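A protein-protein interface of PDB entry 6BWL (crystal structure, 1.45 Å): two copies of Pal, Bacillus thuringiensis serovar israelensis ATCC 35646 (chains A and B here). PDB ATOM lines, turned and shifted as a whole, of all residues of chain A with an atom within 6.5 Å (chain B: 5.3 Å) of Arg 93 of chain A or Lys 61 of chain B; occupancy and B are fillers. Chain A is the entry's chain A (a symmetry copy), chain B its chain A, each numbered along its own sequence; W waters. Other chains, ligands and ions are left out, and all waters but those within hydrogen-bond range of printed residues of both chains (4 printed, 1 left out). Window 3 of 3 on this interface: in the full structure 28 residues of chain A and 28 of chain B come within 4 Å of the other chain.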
ATOM      1  N   SER A  88      10.649  -2.164  -5.848  1.00  0.00           N
ATOM      2  CA  SER A  88      10.954  -3.591  -5.805  1.00  0.00           C
ATOM      3  C   SER A  88      11.835  -3.957  -4.640  1.00  0.00           C
ATOM      4  O   SER A  88      11.778  -5.076  -4.147  1.00  0.00           O
ATOM      5  CB  SER A  88      11.604  -4.042  -7.115  1.00  0.00           C
ATOM      6  OG  SER A  88      13.005  -3.784  -7.180  1.00  0.00           O
ATOM      7  N   ASP A  91       9.351  -3.598  -1.614  1.00  0.00           N
ATOM      8  CA  ASP A  91       8.215  -4.563  -1.682  1.00  0.00           C
ATOM      9  C   ASP A  91       8.504  -5.514  -2.793  1.00  0.00           C
ATOM     10  O   ASP A  91       8.019  -5.392  -3.830  1.00  0.00           O
ATOM     11  CB  ASP A  91       6.880  -3.806  -1.966  1.00  0.00           C
ATOM     12  CG  ASP A  91       5.625  -4.694  -2.024  1.00  0.00           C
ATOM     13  OD1 ASP A  91       4.591  -4.059  -2.184  1.00  0.00           O
ATOM     14  OD2 ASP A  91       5.667  -5.919  -1.948  1.00  0.00           O
ATOM     15  N   ALA A  92       9.323  -6.514  -2.536  1.00  0.00           N
ATOM     16  CA  ALA A  92       9.676  -7.392  -3.655  1.00  0.00           C
ATOM     17  C   ALA A  92       8.502  -8.172  -4.186  1.00  0.00           C
ATOM     18  O   ALA A  92       8.394  -8.403  -5.411  1.00  0.00           O
ATOM     19  CB  ALA A  92      10.841  -8.314  -3.321  1.00  0.00           C
ATOM     20  N   ARG A  93       7.611  -8.628  -3.297  1.00  0.00           N
ATOM     21  CA  ARG A  93       6.530  -9.480  -3.720  1.00  0.00           C
ATOM     22  C   ARG A  93       5.696  -8.848  -4.830  1.00  0.00           C
ATOM     23  O   ARG A  93       5.333  -9.515  -5.793  1.00  0.00           O
ATOM     24  CB  ARG A  93       5.645  -9.852  -2.538  1.00  0.00           C
ATOM     25  CG  ARG A  93       4.387 -10.602  -2.948  1.00  0.00           C
ATOM     26  CD  ARG A  93       3.648 -11.218  -1.771  1.00  0.00           C
ATOM     27  NE  ARG A  93       4.357 -12.363  -1.229  1.00  0.00           N
ATOM     28  CZ  ARG A  93       4.276 -13.602  -1.712  1.00  0.00           C
ATOM     29  NH1 ARG A  93       3.586 -13.857  -2.814  1.00  0.00           N
ATOM     30  NH2 ARG A  93       4.994 -14.567  -1.162  1.00  0.00           N
ATOM     31  N   ALA A  94       5.310  -7.590  -4.683  1.00  0.00           N
ATOM     32  CA  ALA A  94       4.413  -7.035  -5.683  1.00  0.00           C
ATOM     33  C   ALA A  94       5.112  -7.024  -7.050  1.00  0.00           C
ATOM     34  O   ALA A  94       4.497  -7.312  -8.088  1.00  0.00           O
ATOM     35  CB  ALA A  94       3.945  -5.633  -5.284  1.00  0.00           C
ATOM     36  N   THR A  95       6.396  -6.682  -7.074  1.00  0.00           N
ATOM     37  CA  THR A  95       7.137  -6.663  -8.337  1.00  0.00           C
ATOM     38  C   THR A  95       7.262  -8.063  -8.936  1.00  0.00           C
ATOM     39  O   THR A  95       7.067  -8.228 -10.148  1.00  0.00           O
ATOM     40  CB  THR A  95       8.503  -6.010  -8.182  1.00  0.00           C
ATOM     41  OG1 THR A  95       8.321  -4.616  -7.919  1.00  0.00           O
ATOM     42  CG2 THR A  95       9.342  -6.161  -9.429  1.00  0.00           C
ATOM     43  N   PHE A  96       7.549  -9.057  -8.107  1.00  0.00           N
ATOM     44  CA  PHE A  96       7.590 -10.455  -8.537  1.00  0.00           C
ATOM     45  C   PHE A  96       6.274 -10.929  -9.131  1.00  0.00           C
ATOM     46  O   PHE A  96       6.230 -11.623 -10.161  1.00  0.00           O
ATOM     47  CB  PHE A  96       8.068 -11.317  -7.371  1.00  0.00           C
ATOM     48  CG  PHE A  96       8.043 -12.799  -7.624  1.00  0.00           C
ATOM     49  CD1 PHE A  96       8.960 -13.378  -8.491  1.00  0.00           C
ATOM     50  CD2 PHE A  96       7.101 -13.630  -6.999  1.00  0.00           C
ATOM     51  CE1 PHE A  96       8.928 -14.743  -8.707  1.00  0.00           C
ATOM     52  CE2 PHE A  96       7.058 -14.980  -7.222  1.00  0.00           C
ATOM     53  CZ  PHE A  96       7.988 -15.532  -8.097  1.00  0.00           C
ATOM     54  N   GLU A  97       5.196 -10.639  -8.421  1.00  0.00           N
ATOM     55  CA  GLU A  97       3.859 -11.093  -8.848  1.00  0.00           C
ATOM     56  C   GLU A  97       3.500 -10.444 -10.170  1.00  0.00           C
ATOM     57  O   GLU A  97       3.025 -11.107 -11.094  1.00  0.00           O
ATOM     58  CB  GLU A  97       2.801 -10.797  -7.785  1.00  0.00           C
ATOM     59  CG  GLU A  97       2.986 -11.635  -6.539  1.00  0.00           C
ATOM     60  CD  GLU A  97       1.943 -11.366  -5.444  1.00  0.00           C
ATOM     61  OE1 GLU A  97       1.860 -12.202  -4.532  1.00  0.00           O
ATOM     62  OE2 GLU A  97       1.337 -10.304  -5.465  1.00  0.00           O
ATOM     63  N   ASN A  98       3.768  -9.137 -10.310  1.00  0.00           N
ATOM     64  CA  ASN A  98       3.434  -8.467 -11.574  1.00  0.00           C
ATOM     65  C   ASN A  98       4.352  -8.907 -12.719  1.00  0.00           C
ATOM     66  O   ASN A  98       3.874  -9.050 -13.856  1.00  0.00           O
ATOM     67  CB  ASN A  98       3.480  -6.948 -11.405  1.00  0.00           C
ATOM     68  CG  ASN A  98       2.248  -6.439 -10.676  1.00  0.00           C
ATOM     69  OD1 ASN A  98       1.152  -6.525 -11.181  1.00  0.00           O
ATOM     70  ND2 ASN A  98       2.420  -5.987  -9.448  1.00  0.00           N
ATOM     71  N   ILE A 101       5.101 -13.658 -12.296  1.00  0.00           N
ATOM     72  CA  ILE A 101       3.857 -14.432 -12.334  1.00  0.00           C
ATOM     73  C   ILE A 101       2.940 -13.927 -13.447  1.00  0.00           C
ATOM     74  O   ILE A 101       2.391 -14.729 -14.221  1.00  0.00           O
ATOM     75  CB  ILE A 101       3.170 -14.474 -10.979  1.00  0.00           C
ATOM     76  CG1 ILE A 101       4.042 -15.114  -9.910  1.00  0.00           C
ATOM     77  CG2 ILE A 101       1.877 -15.283 -11.105  1.00  0.00           C
ATOM     78  CD1 ILE A 101       3.446 -15.177  -8.516  1.00  0.00           C
ATOM     79  N   PRO A 146      15.229  -6.693  -6.903  1.00  0.00           N
ATOM     80  CA  PRO A 146      14.166  -7.662  -7.234  1.00  0.00           C
ATOM     81  C   PRO A 146      13.467  -7.355  -8.551  1.00  0.00           C
ATOM     82  O   PRO A 146      12.948  -8.300  -9.185  1.00  0.00           O
ATOM     83  CB  PRO A 146      13.236  -7.604  -6.036  1.00  0.00           C
ATOM     84  CG  PRO A 146      14.164  -7.241  -4.949  1.00  0.00           C
ATOM     85  CD  PRO A 146      15.036  -6.180  -5.530  1.00  0.00           C
ATOM     86  N   ILE B  58       5.656 -25.804   0.412  1.00  0.00           N
ATOM     87  CA  ILE B  58       6.284 -24.491   0.254  1.00  0.00           C
ATOM     88  C   ILE B  58       5.413 -23.481  -0.515  1.00  0.00           C
ATOM     89  O   ILE B  58       5.682 -22.281  -0.471  1.00  0.00           O
ATOM     90  CB  ILE B  58       7.707 -24.555  -0.378  1.00  0.00           C
ATOM     91  CG1 ILE B  58       7.619 -25.049  -1.827  1.00  0.00           C
ATOM     92  CG2 ILE B  58       8.592 -25.466   0.460  1.00  0.00           C
ATOM     93  CD1 ILE B  58       8.940 -25.073  -2.552  1.00  0.00           C
ATOM     94  N   LYS B  59       4.393 -23.972  -1.228  1.00  0.00           N
ATOM     95  CA  LYS B  59       3.444 -23.079  -1.884  1.00  0.00           C
ATOM     96  C   LYS B  59       2.396 -22.521  -0.935  1.00  0.00           C
ATOM     97  O   LYS B  59       1.662 -21.637  -1.316  1.00  0.00           O
ATOM     98  CB  LYS B  59       2.717 -23.763  -3.037  1.00  0.00           C
ATOM     99  CG  LYS B  59       3.680 -24.291  -4.112  1.00  0.00           C
ATOM    100  CD  LYS B  59       2.924 -24.831  -5.323  1.00  0.00           C
ATOM    101  CE  LYS B  59       2.009 -25.980  -5.005  1.00  0.00           C
ATOM    102  NZ  LYS B  59       2.694 -27.148  -4.456  1.00  0.00           N
ATOM    103  N   ASP B  60       2.332 -23.035   0.281  1.00  0.00           N
ATOM    104  CA  ASP B  60       1.355 -22.573   1.259  1.00  0.00           C
ATOM    105  C   ASP B  60       1.957 -21.404   2.035  1.00  0.00           C
ATOM    106  O   ASP B  60       2.710 -21.586   2.906  1.00  0.00           O
ATOM    107  CB  ASP B  60       1.016 -23.774   2.155  1.00  0.00           C
ATOM    108  CG  ASP B  60      -0.017 -23.465   3.258  1.00  0.00           C
ATOM    109  OD1 ASP B  60      -0.254 -22.354   3.478  1.00  0.00           O
ATOM    110  OD2 ASP B  60      -0.418 -24.414   3.855  1.00  0.00           O
ATOM    111  N   LYS B  61       1.619 -20.190   1.604  1.00  0.00           N
ATOM    112  CA  LYS B  61       2.259 -18.998   2.121  1.00  0.00           C
ATOM    113  C   LYS B  61       2.061 -18.872   3.641  1.00  0.00           C
ATOM    114  O   LYS B  61       2.960 -18.474   4.364  1.00  0.00           O
ATOM    115  CB  LYS B  61       1.666 -17.738   1.461  1.00  0.00           C
ATOM    116  CG  LYS B  61       1.918 -17.653  -0.039  1.00  0.00           C
ATOM    117  CD  LYS B  61       1.201 -16.427  -0.633  1.00  0.00           C
ATOM    118  CE  LYS B  61       1.304 -15.166   0.209  1.00  0.00           C
ATOM    119  NZ  LYS B  61       0.514 -14.040  -0.396  1.00  0.00           N
ATOM    120  N   LYS B  62       0.871 -19.214   4.100  1.00  0.00           N
ATOM    121  CA  LYS B  62       0.604 -19.060   5.523  1.00  0.00           C
ATOM    122  C   LYS B  62       1.405 -20.037   6.358  1.00  0.00           C
ATOM    123  O   LYS B  62       1.978 -19.696   7.397  1.00  0.00           O
ATOM    124  CB  LYS B  62      -0.887 -19.186   5.817  1.00  0.00           C
ATOM    125  CG  LYS B  62      -1.256 -19.065   7.286  1.00  0.00           C
ATOM    126  CD  LYS B  62      -1.037 -17.670   7.825  1.00  0.00           C
ATOM    127  CE  LYS B  62      -1.944 -17.467   9.036  1.00  0.00           C
ATOM    128  NZ  LYS B  62      -1.342 -16.451   9.948  1.00  0.00           N
ATOM    129  N   LEU B  63       1.485 -21.286   5.905  1.00  0.00           N
ATOM    130  CA  LEU B  63       2.325 -22.261   6.571  1.00  0.00           C
ATOM    131  C   LEU B  63       3.794 -21.847   6.623  1.00  0.00           C
ATOM    132  O   LEU B  63       4.448 -21.917   7.658  1.00  0.00           O
ATOM    133  CB  LEU B  63       2.160 -23.650   5.939  1.00  0.00           C
ATOM    134  CG  LEU B  63       2.986 -24.771   6.570  1.00  0.00           C
ATOM    135  CD1 LEU B  63       2.260 -26.094   6.323  1.00  0.00           C
ATOM    136  CD2 LEU B  63       4.348 -24.897   5.944  1.00  0.00           C
ATOM    137  N   VAL B  64       4.300 -21.343   5.497  1.00  0.00           N
ATOM    138  CA  VAL B  64       5.702 -20.918   5.438  1.00  0.00           C
ATOM    139  C   VAL B  64       5.931 -19.737   6.390  1.00  0.00           C
ATOM    140  O   VAL B  64       6.911 -19.742   7.146  1.00  0.00           O
ATOM    141  CB  VAL B  64       6.070 -20.598   3.988  1.00  0.00           C
ATOM    142  CG1 VAL B  64       7.420 -19.893   3.904  1.00  0.00           C
ATOM    143  CG2 VAL B  64       6.110 -21.891   3.171  1.00  0.00           C
ATOM    144  N   ALA B  65       5.002 -18.787   6.407  1.00  0.00           N
ATOM    145  CA  ALA B  65       5.144 -17.668   7.346  1.00  0.00           C
ATOM    146  C   ALA B  65       5.145 -18.143   8.799  1.00  0.00           C
ATOM    147  O   ALA B  65       6.023 -17.791   9.586  1.00  0.00           O
ATOM    148  CB  ALA B  65       4.065 -16.648   7.128  1.00  0.00           C
ATOM    149  N   GLN B  66       4.176 -19.007   9.142  1.00  0.00           N
ATOM    150  CA  GLN B  66       4.111 -19.507  10.505  1.00  0.00           C
ATOM    151  C   GLN B  66       5.342 -20.294  10.916  1.00  0.00           C
ATOM    152  O   GLN B  66       5.828 -20.222  12.057  1.00  0.00           O
ATOM    153  CB  GLN B  66       2.848 -20.356  10.684  1.00  0.00           C
ATOM    154  CG  GLN B  66       1.570 -19.547  10.669  1.00  0.00           C
ATOM    155  CD  GLN B  66       0.338 -20.427  10.858  1.00  0.00           C
ATOM    156  OE1 GLN B  66       0.285 -21.552  10.375  1.00  0.00           O
ATOM    157  NE2 GLN B  66      -0.669 -19.879  11.489  1.00  0.00           N
ATOM    158  N   PHE B 104      10.333 -18.266  -3.873  1.00  0.00           N
ATOM    159  CA  PHE B 104      10.072 -16.904  -3.487  1.00  0.00           C
ATOM    160  C   PHE B 104       9.410 -16.822  -2.082  1.00  0.00           C
ATOM    161  O   PHE B 104       9.777 -15.996  -1.238  1.00  0.00           O
ATOM    162  CB  PHE B 104       9.210 -16.137  -4.515  1.00  0.00           C
ATOM    163  CG  PHE B 104       9.028 -14.695  -4.119  1.00  0.00           C
ATOM    164  CD1 PHE B 104      10.047 -13.786  -4.356  1.00  0.00           C
ATOM    165  CD2 PHE B 104       7.928 -14.300  -3.381  1.00  0.00           C
ATOM    166  CE1 PHE B 104       9.956 -12.478  -3.923  1.00  0.00           C
ATOM    167  CE2 PHE B 104       7.815 -13.007  -2.952  1.00  0.00           C
ATOM    168  CZ  PHE B 104       8.844 -12.103  -3.208  1.00  0.00           C
ATOM    169  N   ASN B 105       8.455 -17.715  -1.826  1.00  0.00           N
ATOM    170  CA  ASN B 105       7.781 -17.708  -0.517  1.00  0.00           C
ATOM    171  C   ASN B 105       8.804 -17.884   0.603  1.00  0.00           C
ATOM    172  O   ASN B 105       8.742 -17.223   1.628  1.00  0.00           O
ATOM    173  CB  ASN B 105       6.732 -18.795  -0.440  1.00  0.00           C
ATOM    174  CG  ASN B 105       5.546 -18.575  -1.396  1.00  0.00           C
ATOM    175  OD1 ASN B 105       5.285 -17.471  -1.857  1.00  0.00           O
ATOM    176  ND2 ASN B 105       4.835 -19.663  -1.674  1.00  0.00           N
ATOM    177  N   GLU B 108      11.243 -14.740   1.008  1.00  0.00           N
ATOM    178  CA  GLU B 108      10.623 -13.626   1.703  1.00  0.00           C
ATOM    179  C   GLU B 108      10.782 -13.805   3.235  1.00  0.00           C
ATOM    180  O   GLU B 108      11.097 -12.860   3.950  1.00  0.00           O
ATOM    181  CB  GLU B 108       9.138 -13.608   1.288  1.00  0.00           C
ATOM    182  CG  GLU B 108       8.297 -12.524   1.833  1.00  0.00           C
ATOM    183  CD  GLU B 108       6.953 -12.515   1.111  1.00  0.00           C
ATOM    184  OE1 GLU B 108       6.600 -11.523   0.437  1.00  0.00           O
ATOM    185  OE2 GLU B 108       6.265 -13.550   1.180  1.00  0.00           O
ATOM    186  N   TYR B 161      18.073 -10.868  -3.675  1.00  0.00           N
ATOM    187  CA  TYR B 161      18.026 -10.573  -2.245  1.00  0.00           C
ATOM    188  C   TYR B 161      19.410 -10.355  -1.654  1.00  0.00           C
ATOM    189  O   TYR B 161      19.582  -9.515  -0.751  1.00  0.00           O
ATOM    190  CB  TYR B 161      17.254 -11.651  -1.481  1.00  0.00           C
ATOM    191  CG  TYR B 161      15.747 -11.463  -1.478  1.00  0.00           C
ATOM    192  CD1 TYR B 161      15.014 -11.520  -0.316  1.00  0.00           C
ATOM    193  CD2 TYR B 161      15.028 -11.211  -2.647  1.00  0.00           C
ATOM    194  CE1 TYR B 161      13.636 -11.365  -0.306  1.00  0.00           C
ATOM    195  CE2 TYR B 161      13.667 -11.045  -2.637  1.00  0.00           C
ATOM    196  CZ  TYR B 161      12.961 -11.129  -1.466  1.00  0.00           C
ATOM    197  OH  TYR B 161      11.576 -10.976  -1.457  1.00  0.00           O
HETATM  198  O   HOH W   1       3.735 -12.877   1.986  1.00  0.00           O
HETATM  199  O   HOH W   2       3.245 -16.647  -3.381  1.00  0.00           O
HETATM  200  O   HOH W   3      -0.173 -11.621  -2.801  1.00  0.00           O
HETATM  201  O   HOH W   4       8.071  -9.323  -0.331  1.00  0.00           O
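No position is printed for both chains.
Of the 6 pairs that touch across the chains among the printed residues, none has its exchanged pair printed and touching as well.
Of the 13 printed residues of chain B, 5 touch a printed residue of chain A.
Hydrophobic or aromatic side chains of chain B that line the printed part of chain A: Phe 104 and Tyr 161.
Of the 11 printed residues of chain A, 3 touch a printed residue of chain B.
Printed residues of chain A that touch a printed residue of chain B: Ala 92, Arg 93 and Phe 96.
Along chain A the printed residues that touch a printed residue of chain B span positions 92 to 96.
Among the printed residues, Asp or Glu carboxylates within 4 Å of a Lys or Arg side-chain nitrogen of the other chain: Arg 93 of chain A with Glu 108 of chain B (2.9 Å).
CB of Ala 92 of chain A touches OH of Tyr 161 of chain B, at 3.3 Å.
Arg 93 of chain A touches Lys 61 of chain B.
Arg 93 of chain A touches Phe 104 of chain B (CA to CZ, 3.5 Å).
Phe 104 of chain B touches Phe 96 of chain A (CG to CD2, 3.6 Å).
NH2 of Arg 93 of chain A lies within hydrogen-bond range of OD1 of Asn 105 of chain B.
OE2 of Glu 108 of chain B lies within salt-bridge range of NH2 of Arg 93 of chain A (2.9 Å).
Of chain B, only Lys 61 (3.9 Å), Phe 104 (3.5 Å), Asn 105 (3.0 Å) and Glu 108 (2.9 Å) come within 4 Å of Arg 93 of chain A.
Of the printed residues of chain B, Phe 96 of chain A touches Phe 104 (3.6 Å).
Of chain A, only Arg 93 comes within 4 Å of Lys 61 of chain B.
Leu 63 of chain B touches none of the printed residues of chain A.
Val 64 of chain B touches none of the printed residues of chain A.
Of the printed residues of chain A, Phe 104 of chain B touches Arg 93 and Phe 96.
Of the printed residues of chain A, Asn 105 of chain B touches Arg 93 (3.0 Å).
Printed residues of chain A within 4 Å of Glu 108 of chain B: Arg 93 (2.9 Å).
Of the printed residues of chain A, Tyr 161 of chain B touches Ala 92 (3.3 Å).
The nearest residue of chain B that does not touch Arg 93 of chain A is Tyr 161 of chain B (5.0 Å).
The nearest residue of chain A that does not touch Lys 61 of chain B is Glu 97 of chain A (4.7 Å).
Water W2 lies within hydrogen-bond range of OD1 of Asn 105 of chain B and NH1 of Arg 93 of chain A.
Water W3 bridges the side-chain carboxylate (OE1) of Glu 97 of chain A (2.7 Å) and the side-chain amino group (NZ) of Lys 61 of chain B (3.5 Å).
Water W1 bridges OE2 of Glu 108 of chain B and NE of Arg 93 of chain A.
Water W4 bridges OE1 of Glu 108 of chain B and N of Arg 93 of chain A.
O of Phe 96 of chain A is in hydrogen-bond range of N of Ile 101 of chain A.
OE1 of Glu 97 of chain A lies within salt-bridge range of NH1 of Arg 93 of chain A, at 2.9 Å.
The side-chain amide nitrogen of Asn 105 of chain B sits at hydrogen-bond distance from the backbone carbonyl oxygen of Ile 58 of chain B (3.0 Å).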
